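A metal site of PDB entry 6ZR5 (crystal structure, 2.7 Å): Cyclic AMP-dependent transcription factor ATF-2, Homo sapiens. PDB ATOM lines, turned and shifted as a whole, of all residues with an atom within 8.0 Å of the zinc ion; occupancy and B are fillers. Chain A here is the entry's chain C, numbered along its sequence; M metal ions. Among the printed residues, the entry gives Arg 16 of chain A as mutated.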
ATOM      1  N   LEU A   8      -6.341 -14.403  -4.722  1.00  0.00           N
ATOM      2  CA  LEU A   8      -6.826 -13.031  -4.908  1.00  0.00           C
ATOM      3  C   LEU A   8      -6.322 -12.127  -3.792  1.00  0.00           C
ATOM      4  O   LEU A   8      -6.370 -12.487  -2.614  1.00  0.00           O
ATOM      5  CB  LEU A   8      -8.366 -12.989  -4.923  1.00  0.00           C
ATOM      6  N   CYS A   9      -5.828 -10.941  -4.188  1.00  0.00           N
ATOM      7  CA  CYS A   9      -5.520  -9.877  -3.245  1.00  0.00           C
ATOM      8  C   CYS A   9      -6.792  -9.179  -2.843  1.00  0.00           C
ATOM      9  O   CYS A   9      -7.669  -8.934  -3.688  1.00  0.00           O
ATOM     10  CB  CYS A   9      -4.566  -8.847  -3.815  1.00  0.00           C
ATOM     11  SG  CYS A   9      -4.587  -7.230  -2.874  1.00  0.00           S
ATOM     12  N   THR A  10      -6.867  -8.776  -1.576  1.00  0.00           N
ATOM     13  CA  THR A  10      -8.084  -8.228  -0.989  1.00  0.00           C
ATOM     14  C   THR A  10      -8.056  -6.704  -0.811  1.00  0.00           C
ATOM     15  O   THR A  10      -8.990  -6.149  -0.239  1.00  0.00           O
ATOM     16  CB  THR A  10      -8.316  -8.902   0.352  1.00  0.00           C
ATOM     17  OG1 THR A  10      -7.052  -8.983   1.046  1.00  0.00           O
ATOM     18  CG2 THR A  10      -8.861 -10.308   0.146  1.00  0.00           C
ATOM     19  N   ALA A  11      -7.039  -6.035  -1.337  1.00  0.00           N
ATOM     20  CA  ALA A  11      -6.906  -4.594  -1.115  1.00  0.00           C
ATOM     21  C   ALA A  11      -8.039  -3.835  -1.786  1.00  0.00           C
ATOM     22  O   ALA A  11      -8.380  -4.127  -2.941  1.00  0.00           O
ATOM     23  CB  ALA A  11      -5.568  -4.098  -1.632  1.00  0.00           C
ATOM     24  N   PRO A  12      -8.603  -2.822  -1.130  1.00  0.00           N
ATOM     25  CA  PRO A  12      -9.688  -2.052  -1.756  1.00  0.00           C
ATOM     26  C   PRO A  12      -9.187  -1.352  -3.002  1.00  0.00           C
ATOM     27  O   PRO A  12      -8.159  -0.665  -2.974  1.00  0.00           O
ATOM     28  CB  PRO A  12     -10.100  -1.060  -0.663  1.00  0.00           C
ATOM     29  CG  PRO A  12      -9.636  -1.674   0.627  1.00  0.00           C
ATOM     30  CD  PRO A  12      -8.411  -2.467   0.280  1.00  0.00           C
ATOM     31  N   GLY A  13      -9.894  -1.549  -4.105  1.00  0.00           N
ATOM     32  CA  GLY A  13      -9.498  -0.977  -5.383  1.00  0.00           C
ATOM     33  C   GLY A  13      -8.491  -1.773  -6.189  1.00  0.00           C
ATOM     34  O   GLY A  13      -8.062  -1.304  -7.258  1.00  0.00           O
ATOM     35  N   CYS A  14      -8.094  -2.951  -5.733  1.00  0.00           N
ATOM     36  CA  CYS A  14      -7.169  -3.815  -6.457  1.00  0.00           C
ATOM     37  C   CYS A  14      -7.852  -5.160  -6.626  1.00  0.00           C
ATOM     38  O   CYS A  14      -8.195  -5.816  -5.626  1.00  0.00           O
ATOM     39  CB  CYS A  14      -5.822  -3.971  -5.738  1.00  0.00           C
ATOM     40  SG  CYS A  14      -4.409  -4.469  -6.820  1.00  0.00           S
ATOM     41  N   GLY A  15      -8.056  -5.566  -7.865  1.00  0.00           N
ATOM     42  CA  GLY A  15      -8.761  -6.806  -8.127  1.00  0.00           C
ATOM     43  C   GLY A  15      -7.746  -7.842  -8.559  1.00  0.00           C
ATOM     44  O   GLY A  15      -8.089  -8.810  -9.245  1.00  0.00           O
ATOM     45  N   ARG A  16      -6.501  -7.625  -8.152  1.00  0.00           N
ATOM     46  CA  ARG A  16      -5.405  -8.396  -8.702  1.00  0.00           C
ATOM     47  C   ARG A  16      -5.442  -9.813  -8.177  1.00  0.00           C
ATOM     48  O   ARG A  16      -5.828 -10.074  -7.024  1.00  0.00           O
ATOM     49  CB  ARG A  16      -4.046  -7.765  -8.351  1.00  0.00           C
ATOM     50  CG  ARG A  16      -3.688  -6.573  -9.192  1.00  0.00           C
ATOM     51  CD  ARG A  16      -2.218  -6.531  -9.529  1.00  0.00           C
ATOM     52  NE  ARG A  16      -1.751  -7.796 -10.081  1.00  0.00           N
ATOM     53  CZ  ARG A  16      -0.480  -8.059 -10.380  1.00  0.00           C
ATOM     54  NH1 ARG A  16       0.480  -7.155 -10.189  1.00  0.00           N
ATOM     55  NH2 ARG A  16      -0.167  -9.249 -10.886  1.00  0.00           N
ATOM     56  N   ARG A  17      -5.034 -10.736  -9.030  1.00  0.00           N
ATOM     57  CA  ARG A  17      -5.128 -12.155  -8.775  1.00  0.00           C
ATOM     58  C   ARG A  17      -3.799 -12.809  -9.075  1.00  0.00           C
ATOM     59  O   ARG A  17      -3.043 -12.354  -9.934  1.00  0.00           O
ATOM     60  CB  ARG A  17      -6.243 -12.801  -9.619  1.00  0.00           C
ATOM     61  N   PHE A  18      -3.501 -13.863  -8.337  1.00  0.00           N
ATOM     62  CA  PHE A  18      -2.235 -14.557  -8.507  1.00  0.00           C
ATOM     63  C   PHE A  18      -2.487 -16.046  -8.681  1.00  0.00           C
ATOM     64  O   PHE A  18      -3.370 -16.626  -8.030  1.00  0.00           O
ATOM     65  CB  PHE A  18      -1.333 -14.300  -7.318  1.00  0.00           C
ATOM     66  CG  PHE A  18      -0.737 -12.952  -7.329  1.00  0.00           C
ATOM     67  CD1 PHE A  18      -1.487 -11.838  -6.946  1.00  0.00           C
ATOM     68  CD2 PHE A  18       0.562 -12.767  -7.766  1.00  0.00           C
ATOM     69  CE1 PHE A  18      -0.945 -10.591  -6.972  1.00  0.00           C
ATOM     70  CE2 PHE A  18       1.121 -11.520  -7.797  1.00  0.00           C
ATOM     71  CZ  PHE A  18       0.365 -10.422  -7.409  1.00  0.00           C
ATOM     72  N   LEU A  24       1.440 -13.955  -4.449  1.00  0.00           N
ATOM     73  CA  LEU A  24       0.481 -13.104  -3.744  1.00  0.00           C
ATOM     74  C   LEU A  24       1.062 -12.594  -2.432  1.00  0.00           C
ATOM     75  O   LEU A  24       0.689 -11.511  -1.967  1.00  0.00           O
ATOM     76  CB  LEU A  24      -0.831 -13.875  -3.499  1.00  0.00           C
ATOM     77  CG  LEU A  24      -1.975 -13.264  -2.654  1.00  0.00           C
ATOM     78  CD1 LEU A  24      -3.318 -13.788  -3.116  1.00  0.00           C
ATOM     79  CD2 LEU A  24      -1.828 -13.507  -1.142  1.00  0.00           C
ATOM     80  N   HIS A  27       2.866  -9.484  -2.959  1.00  0.00           N
ATOM     81  CA  HIS A  27       1.921  -8.455  -3.359  1.00  0.00           C
ATOM     82  C   HIS A  27       1.154  -7.878  -2.177  1.00  0.00           C
ATOM     83  O   HIS A  27       0.883  -6.676  -2.140  1.00  0.00           O
ATOM     84  CB  HIS A  27       0.933  -8.965  -4.394  1.00  0.00           C
ATOM     85  CG  HIS A  27       0.013  -7.896  -4.884  1.00  0.00           C
ATOM     86  ND1 HIS A  27       0.357  -7.044  -5.921  1.00  0.00           N
ATOM     87  CD2 HIS A  27      -1.214  -7.511  -4.467  1.00  0.00           C
ATOM     88  CE1 HIS A  27      -0.633  -6.187  -6.128  1.00  0.00           C
ATOM     89  NE2 HIS A  27      -1.597  -6.447  -5.260  1.00  0.00           N
ATOM     90  N   LYS A  28       0.732  -8.730  -1.217  1.00  0.00           N
ATOM     91  CA  LYS A  28       0.010  -8.171  -0.066  1.00  0.00           C
ATOM     92  C   LYS A  28       0.934  -7.331   0.784  1.00  0.00           C
ATOM     93  O   LYS A  28       0.535  -6.289   1.316  1.00  0.00           O
ATOM     94  CB  LYS A  28      -0.638  -9.291   0.752  1.00  0.00           C
ATOM     95  N   LYS A  30       3.360  -5.594  -0.259  1.00  0.00           N
ATOM     96  CA  LYS A  30       3.607  -4.353  -0.955  1.00  0.00           C
ATOM     97  C   LYS A  30       2.551  -3.291  -0.646  1.00  0.00           C
ATOM     98  O   LYS A  30       2.856  -2.090  -0.593  1.00  0.00           O
ATOM     99  CB  LYS A  30       3.647  -4.543  -2.470  1.00  0.00           C
ATOM    100  CG  LYS A  30       4.918  -5.232  -2.927  1.00  0.00           C
ATOM    101  CD  LYS A  30       4.896  -5.442  -4.428  1.00  0.00           C
ATOM    102  CE  LYS A  30       6.198  -6.001  -4.982  1.00  0.00           C
ATOM    103  NZ  LYS A  30       6.140  -6.237  -6.484  1.00  0.00           N
ATOM    104  N   HIS A  31       1.288  -3.720  -0.492  1.00  0.00           N
ATOM    105  CA  HIS A  31       0.200  -2.848  -0.034  1.00  0.00           C
ATOM    106  C   HIS A  31       0.416  -2.365   1.386  1.00  0.00           C
ATOM    107  O   HIS A  31       0.012  -1.235   1.728  1.00  0.00           O
ATOM    108  CB  HIS A  31      -1.121  -3.603  -0.157  1.00  0.00           C
ATOM    109  CG  HIS A  31      -1.716  -3.495  -1.523  1.00  0.00           C
ATOM    110  ND1 HIS A  31      -1.808  -2.289  -2.191  1.00  0.00           N
ATOM    111  CD2 HIS A  31      -2.225  -4.441  -2.352  1.00  0.00           C
ATOM    112  CE1 HIS A  31      -2.364  -2.491  -3.378  1.00  0.00           C
ATOM    113  NE2 HIS A  31      -2.627  -3.788  -3.494  1.00  0.00           N
HETATM  114 ZN    ZN M   1      -3.522  -5.765  -4.520  1.00  0.00          ZN
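The backbone carbonyl oxygen of Arg 16 is in hydrogen-bond range of the backbone NH of Cys 9.
The side-chain sulfur (SG) of Cys 9 sits close to the backbone NH (N) of Ala 11 (3.1 Å).
CB of Ala 11 touches the zinc ion, at 3.9 Å.
Within 4 Å of the zinc ion: Cys 9, Ala 11, Cys 14, His 27 and His 31.
The nearest printed residue that does not touch the zinc ion is Arg 16 (4.4 Å).
The zinc ion is bound by NE2 of His 27, at 2.2 Å.
NE2 of His 31 is bound to the zinc ion (2.4 Å).
SG of Cys 9 binds the zinc ion (2.4 Å).
SG of Cys 14 binds the zinc ion.
The zinc ion has four donor atoms within binding distance.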
